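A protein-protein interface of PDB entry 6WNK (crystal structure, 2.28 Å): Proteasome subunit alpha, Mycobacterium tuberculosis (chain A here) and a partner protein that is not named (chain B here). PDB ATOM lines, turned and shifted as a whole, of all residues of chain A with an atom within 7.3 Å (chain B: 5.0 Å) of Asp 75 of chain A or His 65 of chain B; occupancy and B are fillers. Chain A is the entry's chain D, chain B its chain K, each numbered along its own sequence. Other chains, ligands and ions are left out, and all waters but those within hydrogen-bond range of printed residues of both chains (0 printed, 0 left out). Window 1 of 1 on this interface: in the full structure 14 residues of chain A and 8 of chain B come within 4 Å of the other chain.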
ATOM      1  N   LEU A  48     -26.405 -23.571 -14.295  1.00  0.00           N
ATOM      2  CA  LEU A  48     -25.382 -24.172 -13.448  1.00  0.00           C
ATOM      3  C   LEU A  48     -24.242 -24.769 -14.257  1.00  0.00           C
ATOM      4  O   LEU A  48     -23.071 -24.551 -13.937  1.00  0.00           O
ATOM      5  CB  LEU A  48     -25.989 -25.260 -12.551  1.00  0.00           C
ATOM      6  CG  LEU A  48     -26.860 -24.861 -11.360  1.00  0.00           C
ATOM      7  CD1 LEU A  48     -27.279 -26.101 -10.585  1.00  0.00           C
ATOM      8  CD2 LEU A  48     -26.148 -23.875 -10.447  1.00  0.00           C
ATOM      9  N   TYR A  49     -24.560 -25.530 -15.300  1.00  0.00           N
ATOM     10  CA  TYR A  49     -23.551 -26.136 -16.157  1.00  0.00           C
ATOM     11  C   TYR A  49     -24.152 -26.299 -17.550  1.00  0.00           C
ATOM     12  O   TYR A  49     -25.234 -25.780 -17.837  1.00  0.00           O
ATOM     13  CB  TYR A  49     -23.053 -27.457 -15.559  1.00  0.00           C
ATOM     14  CG  TYR A  49     -21.589 -27.716 -15.825  1.00  0.00           C
ATOM     15  CD1 TYR A  49     -20.612 -26.856 -15.337  1.00  0.00           C
ATOM     16  CD2 TYR A  49     -21.182 -28.821 -16.557  1.00  0.00           C
ATOM     17  CE1 TYR A  49     -19.270 -27.087 -15.576  1.00  0.00           C
ATOM     18  CE2 TYR A  49     -19.845 -29.064 -16.799  1.00  0.00           C
ATOM     19  CZ  TYR A  49     -18.893 -28.192 -16.309  1.00  0.00           C
ATOM     20  OH  TYR A  49     -17.559 -28.427 -16.547  1.00  0.00           O
ATOM     21  N   ASP A  50     -23.438 -27.021 -18.418  1.00  0.00           N
ATOM     22  CA  ASP A  50     -23.830 -27.135 -19.820  1.00  0.00           C
ATOM     23  C   ASP A  50     -25.285 -27.566 -19.958  1.00  0.00           C
ATOM     24  O   ASP A  50     -26.093 -26.894 -20.611  1.00  0.00           O
ATOM     25  CB  ASP A  50     -22.912 -28.126 -20.541  1.00  0.00           C
ATOM     26  CG  ASP A  50     -21.467 -27.677 -20.566  1.00  0.00           C
ATOM     27  OD1 ASP A  50     -21.224 -26.459 -20.452  1.00  0.00           O
ATOM     28  OD2 ASP A  50     -20.578 -28.544 -20.703  1.00  0.00           O
ATOM     29  N   ARG A  68     -24.520 -19.781  -6.281  1.00  0.00           N
ATOM     30  CA  ARG A  68     -23.089 -19.591  -6.493  1.00  0.00           C
ATOM     31  C   ARG A  68     -22.294 -20.794  -6.000  1.00  0.00           C
ATOM     32  O   ARG A  68     -21.345 -21.230  -6.662  1.00  0.00           O
ATOM     33  CB  ARG A  68     -22.629 -18.306  -5.802  1.00  0.00           C
ATOM     34  CG  ARG A  68     -23.336 -17.054  -6.310  1.00  0.00           C
ATOM     35  CD  ARG A  68     -22.960 -15.810  -5.514  1.00  0.00           C
ATOM     36  NE  ARG A  68     -23.607 -14.615  -6.054  1.00  0.00           N
ATOM     37  CZ  ARG A  68     -23.062 -13.802  -6.952  1.00  0.00           C
ATOM     38  NH1 ARG A  68     -21.841 -14.039  -7.419  1.00  0.00           N
ATOM     39  NH2 ARG A  68     -23.739 -12.746  -7.384  1.00  0.00           N
ATOM     40  N   GLY A  70     -23.284 -23.801  -6.045  1.00  0.00           N
ATOM     41  CA  GLY A  70     -23.453 -24.872  -7.015  1.00  0.00           C
ATOM     42  C   GLY A  70     -22.624 -24.653  -8.265  1.00  0.00           C
ATOM     43  O   GLY A  70     -22.039 -25.597  -8.807  1.00  0.00           O
ATOM     44  N   ILE A  71     -22.568 -23.410  -8.744  1.00  0.00           N
ATOM     45  CA  ILE A  71     -21.725 -23.093  -9.892  1.00  0.00           C
ATOM     46  C   ILE A  71     -20.266 -23.393  -9.578  1.00  0.00           C
ATOM     47  O   ILE A  71     -19.539 -23.956 -10.406  1.00  0.00           O
ATOM     48  CB  ILE A  71     -21.929 -21.626 -10.314  1.00  0.00           C
ATOM     49  CG1 ILE A  71     -23.365 -21.401 -10.791  1.00  0.00           C
ATOM     50  CG2 ILE A  71     -20.936 -21.238 -11.402  1.00  0.00           C
ATOM     51  CD1 ILE A  71     -23.654 -19.973 -11.197  1.00  0.00           C
ATOM     52  N   GLN A  72     -19.818 -23.032  -8.372  1.00  0.00           N
ATOM     53  CA  GLN A  72     -18.454 -23.351  -7.960  1.00  0.00           C
ATOM     54  C   GLN A  72     -18.214 -24.853  -7.986  1.00  0.00           C
ATOM     55  O   GLN A  72     -17.197 -25.322  -8.508  1.00  0.00           O
ATOM     56  CB  GLN A  72     -18.180 -22.791  -6.564  1.00  0.00           C
ATOM     57  CG  GLN A  72     -18.144 -21.276  -6.488  1.00  0.00           C
ATOM     58  CD  GLN A  72     -16.801 -20.702  -6.887  1.00  0.00           C
ATOM     59  OE1 GLN A  72     -15.853 -21.442  -7.159  1.00  0.00           O
ATOM     60  NE2 GLN A  72     -16.710 -19.375  -6.920  1.00  0.00           N
ATOM     61  N   PHE A  73     -19.146 -25.628  -7.424  1.00  0.00           N
ATOM     62  CA  PHE A  73     -18.972 -27.077  -7.384  1.00  0.00           C
ATOM     63  C   PHE A  73     -18.935 -27.665  -8.788  1.00  0.00           C
ATOM     64  O   PHE A  73     -18.163 -28.593  -9.058  1.00  0.00           O
ATOM     65  CB  PHE A  73     -20.088 -27.720  -6.562  1.00  0.00           C
ATOM     66  CG  PHE A  73     -20.019 -29.220  -6.518  1.00  0.00           C
ATOM     67  CD1 PHE A  73     -20.650 -29.987  -7.485  1.00  0.00           C
ATOM     68  CD2 PHE A  73     -19.321 -29.863  -5.510  1.00  0.00           C
ATOM     69  CE1 PHE A  73     -20.580 -31.368  -7.450  1.00  0.00           C
ATOM     70  CE2 PHE A  73     -19.249 -31.245  -5.469  1.00  0.00           C
ATOM     71  CZ  PHE A  73     -19.877 -31.997  -6.441  1.00  0.00           C
ATOM     72  N   ALA A  74     -19.761 -27.138  -9.694  1.00  0.00           N
ATOM     73  CA  ALA A  74     -19.846 -27.698 -11.038  1.00  0.00           C
ATOM     74  C   ALA A  74     -18.578 -27.419 -11.834  1.00  0.00           C
ATOM     75  O   ALA A  74     -17.972 -28.341 -12.395  1.00  0.00           O
ATOM     76  CB  ALA A  74     -21.070 -27.140 -11.766  1.00  0.00           C
ATOM     77  N   ASP A  75     -18.167 -26.149 -11.899  1.00  0.00           N
ATOM     78  CA  ASP A  75     -16.966 -25.792 -12.649  1.00  0.00           C
ATOM     79  C   ASP A  75     -15.741 -26.507 -12.100  1.00  0.00           C
ATOM     80  O   ASP A  75     -14.870 -26.938 -12.865  1.00  0.00           O
ATOM     81  CB  ASP A  75     -16.763 -24.279 -12.629  1.00  0.00           C
ATOM     82  CG  ASP A  75     -17.791 -23.545 -13.465  1.00  0.00           C
ATOM     83  OD1 ASP A  75     -18.449 -24.198 -14.305  1.00  0.00           O
ATOM     84  OD2 ASP A  75     -17.936 -22.319 -13.291  1.00  0.00           O
ATOM     85  N   THR A  76     -15.669 -26.668 -10.776  1.00  0.00           N
ATOM     86  CA  THR A  76     -14.529 -27.355 -10.175  1.00  0.00           C
ATOM     87  C   THR A  76     -14.532 -28.843 -10.520  1.00  0.00           C
ATOM     88  O   THR A  76     -13.479 -29.412 -10.838  1.00  0.00           O
ATOM     89  CB  THR A  76     -14.531 -27.139  -8.661  1.00  0.00           C
ATOM     90  OG1 THR A  76     -14.312 -25.750  -8.379  1.00  0.00           O
ATOM     91  CG2 THR A  76     -13.437 -27.959  -7.995  1.00  0.00           C
ATOM     92  N   ARG A  77     -15.702 -29.490 -10.467  1.00  0.00           N
ATOM     93  CA  ARG A  77     -15.789 -30.891 -10.872  1.00  0.00           C
ATOM     94  C   ARG A  77     -15.466 -31.060 -12.349  1.00  0.00           C
ATOM     95  O   ARG A  77     -14.730 -31.977 -12.733  1.00  0.00           O
ATOM     96  CB  ARG A  77     -17.182 -31.446 -10.571  1.00  0.00           C
ATOM     97  CG  ARG A  77     -17.339 -32.045  -9.186  1.00  0.00           C
ATOM     98  CD  ARG A  77     -16.674 -33.410  -9.089  1.00  0.00           C
ATOM     99  NE  ARG A  77     -16.661 -33.901  -7.714  1.00  0.00           N
ATOM    100  CZ  ARG A  77     -17.578 -34.710  -7.195  1.00  0.00           C
ATOM    101  NH1 ARG A  77     -18.588 -35.139  -7.940  1.00  0.00           N
ATOM    102  NH2 ARG A  77     -17.481 -35.097  -5.930  1.00  0.00           N
ATOM    103  N   GLY A  78     -16.007 -30.178 -13.193  1.00  0.00           N
ATOM    104  CA  GLY A  78     -15.757 -30.276 -14.620  1.00  0.00           C
ATOM    105  C   GLY A  78     -14.312 -30.025 -14.999  1.00  0.00           C
ATOM    106  O   GLY A  78     -13.836 -30.542 -16.015  1.00  0.00           O
ATOM    107  N   TYR A  79     -13.594 -29.227 -14.200  1.00  0.00           N
ATOM    108  CA  TYR A  79     -12.178 -29.004 -14.471  1.00  0.00           C
ATOM    109  C   TYR A  79     -11.314 -30.114 -13.885  1.00  0.00           C
ATOM    110  O   TYR A  79     -10.351 -30.554 -14.521  1.00  0.00           O
ATOM    111  CB  TYR A  79     -11.732 -27.645 -13.928  1.00  0.00           C
ATOM    112  CG  TYR A  79     -10.278 -27.346 -14.222  1.00  0.00           C
ATOM    113  CD1 TYR A  79      -9.874 -26.965 -15.494  1.00  0.00           C
ATOM    114  CD2 TYR A  79      -9.306 -27.459 -13.233  1.00  0.00           C
ATOM    115  CE1 TYR A  79      -8.547 -26.697 -15.777  1.00  0.00           C
ATOM    116  CE2 TYR A  79      -7.971 -27.189 -13.506  1.00  0.00           C
ATOM    117  CZ  TYR A  79      -7.600 -26.811 -14.782  1.00  0.00           C
ATOM    118  OH  TYR A  79      -6.278 -26.543 -15.071  1.00  0.00           O
ATOM    119  N   ALA A  80     -11.638 -30.576 -12.675  1.00  0.00           N
ATOM    120  CA  ALA A  80     -10.853 -31.639 -12.058  1.00  0.00           C
ATOM    121  C   ALA A  80     -10.945 -32.947 -12.836  1.00  0.00           C
ATOM    122  O   ALA A  80      -9.993 -33.735 -12.836  1.00  0.00           O
ATOM    123  CB  ALA A  80     -11.306 -31.849 -10.614  1.00  0.00           C
ATOM    124  N   TYR A  81     -12.078 -33.199 -13.497  1.00  0.00           N
ATOM    125  CA  TYR A  81     -12.251 -34.400 -14.294  1.00  0.00           C
ATOM    126  C   TYR A  81     -12.578 -33.947 -15.708  1.00  0.00           C
ATOM    127  O   TYR A  81     -11.688 -33.469 -16.427  1.00  0.00           O
ATOM    128  CB  TYR A  81     -13.311 -35.311 -13.662  1.00  0.00           C
ATOM    129  CG  TYR A  81     -13.000 -35.678 -12.233  1.00  0.00           C
ATOM    130  CD1 TYR A  81     -12.213 -36.781 -11.940  1.00  0.00           C
ATOM    131  CD2 TYR A  81     -13.469 -34.908 -11.176  1.00  0.00           C
ATOM    132  CE1 TYR A  81     -11.911 -37.116 -10.638  1.00  0.00           C
ATOM    133  CE2 TYR A  81     -13.171 -35.233  -9.870  1.00  0.00           C
ATOM    134  CZ  TYR A  81     -12.391 -36.338  -9.611  1.00  0.00           C
ATOM    135  OH  TYR A  81     -12.088 -36.674  -8.319  1.00  0.00           O
ATOM    136  N   ARG A  83     -15.981 -32.167 -18.310  1.00  0.00           N
ATOM    137  CA  ARG A  83     -17.280 -31.503 -18.278  1.00  0.00           C
ATOM    138  C   ARG A  83     -18.428 -32.506 -18.211  1.00  0.00           C
ATOM    139  O   ARG A  83     -19.424 -32.274 -17.514  1.00  0.00           O
ATOM    140  CB  ARG A  83     -17.437 -30.601 -19.499  1.00  0.00           C
ATOM    141  CG  ARG A  83     -16.248 -29.699 -19.768  1.00  0.00           C
ATOM    142  CD  ARG A  83     -16.613 -28.623 -20.769  1.00  0.00           C
ATOM    143  NE  ARG A  83     -17.681 -27.766 -20.262  1.00  0.00           N
ATOM    144  CZ  ARG A  83     -17.483 -26.723 -19.462  1.00  0.00           C
ATOM    145  NH1 ARG A  83     -16.256 -26.405 -19.078  1.00  0.00           N
ATOM    146  NH2 ARG A  83     -18.512 -25.999 -19.047  1.00  0.00           N
ATOM    147  N   VAL A  86     -20.034 -33.910 -14.854  1.00  0.00           N
ATOM    148  CA  VAL A  86     -20.955 -33.108 -14.058  1.00  0.00           C
ATOM    149  C   VAL A  86     -22.379 -33.500 -14.433  1.00  0.00           C
ATOM    150  O   VAL A  86     -22.794 -33.323 -15.583  1.00  0.00           O
ATOM    151  CB  VAL A  86     -20.720 -31.608 -14.286  1.00  0.00           C
ATOM    152  CG1 VAL A  86     -21.765 -30.785 -13.546  1.00  0.00           C
ATOM    153  CG2 VAL A  86     -19.313 -31.215 -13.856  1.00  0.00           C
ATOM    154  N   LEU A  91     -25.289 -32.478  -8.586  1.00  0.00           N
ATOM    155  CA  LEU A  91     -25.586 -31.168  -8.017  1.00  0.00           C
ATOM    156  C   LEU A  91     -26.752 -31.233  -7.037  1.00  0.00           C
ATOM    157  O   LEU A  91     -26.732 -30.564  -5.999  1.00  0.00           O
ATOM    158  CB  LEU A  91     -25.861 -30.167  -9.136  1.00  0.00           C
ATOM    159  CG  LEU A  91     -24.571 -29.566  -9.702  1.00  0.00           C
ATOM    160  CD1 LEU A  91     -24.788 -28.971 -11.080  1.00  0.00           C
ATOM    161  CD2 LEU A  91     -24.028 -28.511  -8.743  1.00  0.00           C
ATOM    162  N   ALA B  60     -10.551 -20.830 -20.165  1.00  0.00           N
ATOM    163  CA  ALA B  60     -11.929 -20.941 -20.636  1.00  0.00           C
ATOM    164  C   ALA B  60     -12.890 -21.170 -19.476  1.00  0.00           C
ATOM    165  O   ALA B  60     -13.970 -20.567 -19.423  1.00  0.00           O
ATOM    166  CB  ALA B  60     -12.046 -22.071 -21.659  1.00  0.00           C
ATOM    167  N   VAL B  61     -12.506 -22.033 -18.531  1.00  0.00           N
ATOM    168  CA  VAL B  61     -13.342 -22.277 -17.359  1.00  0.00           C
ATOM    169  C   VAL B  61     -13.524 -20.994 -16.553  1.00  0.00           C
ATOM    170  O   VAL B  61     -14.624 -20.700 -16.072  1.00  0.00           O
ATOM    171  CB  VAL B  61     -12.743 -23.412 -16.506  1.00  0.00           C
ATOM    172  CG1 VAL B  61     -13.399 -23.460 -15.141  1.00  0.00           C
ATOM    173  CG2 VAL B  61     -12.903 -24.756 -17.221  1.00  0.00           C
ATOM    174  N   GLU B  62     -12.459 -20.198 -16.413  1.00  0.00           N
ATOM    175  CA  GLU B  62     -12.552 -18.980 -15.611  1.00  0.00           C
ATOM    176  C   GLU B  62     -13.517 -17.977 -16.235  1.00  0.00           C
ATOM    177  O   GLU B  62     -14.376 -17.420 -15.542  1.00  0.00           O
ATOM    178  CB  GLU B  62     -11.166 -18.353 -15.422  1.00  0.00           C
ATOM    179  CG  GLU B  62     -11.144 -17.210 -14.399  1.00  0.00           C
ATOM    180  CD  GLU B  62      -9.767 -16.574 -14.224  1.00  0.00           C
ATOM    181  OE1 GLU B  62      -9.704 -15.365 -13.897  1.00  0.00           O
ATOM    182  OE2 GLU B  62      -8.754 -17.279 -14.407  1.00  0.00           O
ATOM    183  N   LEU B  63     -13.393 -17.734 -17.544  1.00  0.00           N
ATOM    184  CA  LEU B  63     -14.274 -16.771 -18.203  1.00  0.00           C
ATOM    185  C   LEU B  63     -15.740 -17.171 -18.065  1.00  0.00           C
ATOM    186  O   LEU B  63     -16.600 -16.325 -17.786  1.00  0.00           O
ATOM    187  CB  LEU B  63     -13.899 -16.632 -19.677  1.00  0.00           C
ATOM    188  CG  LEU B  63     -12.564 -15.977 -20.039  1.00  0.00           C
ATOM    189  CD1 LEU B  63     -12.461 -15.797 -21.543  1.00  0.00           C
ATOM    190  CD2 LEU B  63     -12.401 -14.643 -19.332  1.00  0.00           C
ATOM    191  N   GLU B  64     -16.045 -18.456 -18.262  1.00  0.00           N
ATOM    192  CA  GLU B  64     -17.423 -18.911 -18.120  1.00  0.00           C
ATOM    193  C   GLU B  64     -17.855 -18.919 -16.660  1.00  0.00           C
ATOM    194  O   GLU B  64     -19.032 -18.685 -16.361  1.00  0.00           O
ATOM    195  CB  GLU B  64     -17.588 -20.300 -18.738  1.00  0.00           C
ATOM    196  CG  GLU B  64     -19.008 -20.853 -18.648  1.00  0.00           C
ATOM    197  CD  GLU B  64     -19.161 -22.209 -19.311  1.00  0.00           C
ATOM    198  OE1 GLU B  64     -18.765 -22.343 -20.491  1.00  0.00           O
ATOM    199  OE2 GLU B  64     -19.667 -23.142 -18.646  1.00  0.00           O
ATOM    200  N   HIS B  65     -16.917 -19.175 -15.745  1.00  0.00           N
ATOM    201  CA  HIS B  65     -17.224 -19.132 -14.319  1.00  0.00           C
ATOM    202  C   HIS B  65     -17.745 -17.760 -13.916  1.00  0.00           C
ATOM    203  O   HIS B  65     -18.748 -17.648 -13.198  1.00  0.00           O
ATOM    204  CB  HIS B  65     -15.977 -19.497 -13.516  1.00  0.00           C
ATOM    205  CG  HIS B  65     -16.210 -19.604 -12.041  1.00  0.00           C
ATOM    206  ND1 HIS B  65     -17.000 -20.585 -11.481  1.00  0.00           N
ATOM    207  CD2 HIS B  65     -15.739 -18.863 -11.010  1.00  0.00           C
ATOM    208  CE1 HIS B  65     -17.013 -20.438 -10.168  1.00  0.00           C
ATOM    209  NE2 HIS B  65     -16.254 -19.402  -9.856  1.00  0.00           N
ATOM    210  N   TYR B  66     -17.077 -16.699 -14.373  1.00  0.00           N
ATOM    211  CA  TYR B  66     -17.547 -15.352 -14.071  1.00  0.00           C
ATOM    212  C   TYR B  66     -18.904 -15.089 -14.709  1.00  0.00           C
ATOM    213  O   TYR B  66     -19.784 -14.484 -14.085  1.00  0.00           O
ATOM    214  CB  TYR B  66     -16.525 -14.318 -14.547  1.00  0.00           C
ATOM    215  CG  TYR B  66     -16.895 -12.888 -14.213  1.00  0.00           C
ATOM    216  CD1 TYR B  66     -17.775 -12.169 -15.014  1.00  0.00           C
ATOM    217  CD2 TYR B  66     -16.353 -12.249 -13.101  1.00  0.00           C
ATOM    218  CE1 TYR B  66     -18.115 -10.865 -14.714  1.00  0.00           C
ATOM    219  CE2 TYR B  66     -16.685 -10.942 -12.794  1.00  0.00           C
ATOM    220  CZ  TYR B  66     -17.568 -10.255 -13.604  1.00  0.00           C
ATOM    221  OH  TYR B  66     -17.913  -8.952 -13.310  1.00  0.00           O
ATOM    222  N   GLU B  67     -19.087 -15.524 -15.959  1.00  0.00           N
ATOM    223  CA  GLU B  67     -20.338 -15.258 -16.661  1.00  0.00           C
ATOM    224  C   GLU B  67     -21.526 -15.884 -15.937  1.00  0.00           C
ATOM    225  O   GLU B  67     -22.590 -15.264 -15.825  1.00  0.00           O
ATOM    226  CB  GLU B  67     -20.251 -15.773 -18.098  1.00  0.00           C
ATOM    227  CG  GLU B  67     -21.301 -15.191 -19.032  1.00  0.00           C
ATOM    228  CD  GLU B  67     -21.331 -15.880 -20.388  1.00  0.00           C
ATOM    229  OE1 GLU B  67     -22.436 -16.038 -20.951  1.00  0.00           O
ATOM    230  OE2 GLU B  67     -20.255 -16.265 -20.890  1.00  0.00           O
ATOM    231  N   LYS B  68     -21.359 -17.107 -15.427  1.00  0.00           N
ATOM    232  CA  LYS B  68     -22.460 -17.766 -14.733  1.00  0.00           C
ATOM    233  C   LYS B  68     -22.701 -17.166 -13.353  1.00  0.00           C
ATOM    234  O   LYS B  68     -23.851 -17.085 -12.908  1.00  0.00           O
ATOM    235  CB  LYS B  68     -22.188 -19.273 -14.626  1.00  0.00           C
ATOM    236  CG  LYS B  68     -22.138 -19.999 -15.974  1.00  0.00           C
ATOM    237  CD  LYS B  68     -22.009 -21.512 -15.817  1.00  0.00           C
ATOM    238  CE  LYS B  68     -20.639 -21.922 -15.304  1.00  0.00           C
ATOM    239  NZ  LYS B  68     -20.458 -23.404 -15.296  1.00  0.00           N
ATOM    240  N   LEU B  69     -21.643 -16.727 -12.667  1.00  0.00           N
ATOM    241  CA  LEU B  69     -21.826 -16.145 -11.343  1.00  0.00           C
ATOM    242  C   LEU B  69     -22.472 -14.768 -11.424  1.00  0.00           C
ATOM    243  O   LEU B  69     -23.295 -14.415 -10.574  1.00  0.00           O
ATOM    244  CB  LEU B  69     -20.488 -16.054 -10.611  1.00  0.00           C
ATOM    245  CG  LEU B  69     -19.829 -17.347 -10.130  1.00  0.00           C
ATOM    246  CD1 LEU B  69     -18.495 -17.032  -9.472  1.00  0.00           C
ATOM    247  CD2 LEU B  69     -20.739 -18.099  -9.171  1.00  0.00           C
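Asp 75 of chain A touches two residues of chain B.
Of the printed residues of chain A, His 65 of chain B touches Ile 71 (3.99 Å), Gln 72 (3.0 Å) and Asp 75 (2.7 Å).
Printed residues of chain A within 4 Å of Lys 68 of chain B: Leu 48, Tyr 49, Ile 71 and Asp 75.
Of the printed residues of chain A, Leu 69 of chain B touches Arg 68, Ile 71 and Gln 72.
Of the printed residues of chain B, Tyr 49 of chain A touches Lys 68 (3.5 Å).
The nearest residue of chain B that does not touch Asp 75 of chain A is Val 61 of chain B (4.3 Å).
The nearest printed residue of chain A that does not touch His 65 of chain B is Arg 68 of chain A (5.6 Å).
The nearest printed residue of chain B that does not touch Arg 83 of chain A is Val 61 of chain B (4.2 Å).
Among the printed residues, pairs that only touch across the chains: Ile 71 of chain A with Lys 68 of chain B, Tyr 49 of chain A with Lys 68 of chain B, Ile 71 of chain A with Leu 69 of chain B, Gln 72 of chain A with Leu 69 of chain B and Ile 71 of chain A with His 65 of chain B.
OH of Tyr 49 of chain A sits close to NH1 of Arg 83 of chain A (3.5 Å).
NE of Arg 83 of chain A lies within salt-bridge range of OD2 of Asp 50 of chain A, at 3.0 Å.
The backbone carbonyl oxygen (O) of Gln 72 of chain A lies within hydrogen-bond range of the side-chain hydroxyl (OG1) of Thr 76 of chain A (2.9 Å).
The side-chain carboxylate (OE2) of Glu 64 of chain B lies within salt-bridge range of the side-chain amino group (NZ) of Lys 68 of chain B (3.5 Å).
NZ of Lys 68 of chain B lies within hydrogen-bond range of O of Leu 48 of chain A, at 3.2 Å.
The guanidinium group of Arg 68 of chain A lies within hydrogen-bond range of the backbone carbonyl oxygen of Leu 69 of chain B.
The side-chain amide nitrogen (NE2) of Gln 72 of chain A sits at hydrogen-bond distance from a ring nitrogen (NE2) of His 65 of chain B, 3.0 Å away.
A ring nitrogen (ND1) of His 65 of chain B is in hydrogen-bond range of the side-chain carboxylate of Asp 75 of chain A.
The side-chain amino group (NZ) of Lys 68 of chain B is in salt-bridge range of the side-chain carboxylate (OD2) of Asp 75 of chain A (3.4 Å).
OE2 of Glu 64 of chain B lies within salt-bridge range of NH2 of Arg 83 of chain A.
Printed residues of chain A that touch a printed residue of chain B: Leu 48, Tyr 49, Arg 68, Ile 71, Gln 72, Asp 75 and Arg 83.
Hydrophobic or aromatic side chains of chain A that line the printed part of chain B: Tyr 49 and Ile 71.
Printed residues of chain B that touch a printed residue of chain A: Glu 64, His 65, Lys 68 and Leu 69.
Hydrophobic or aromatic side chains of chain B within 4 Å of the printed part of chain A: His 65 and Leu 69.
Along chain B the printed residues that touch a printed residue of chain A span positions 64 to 69.
Among the printed residues, 11 pairs touch across the chains.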
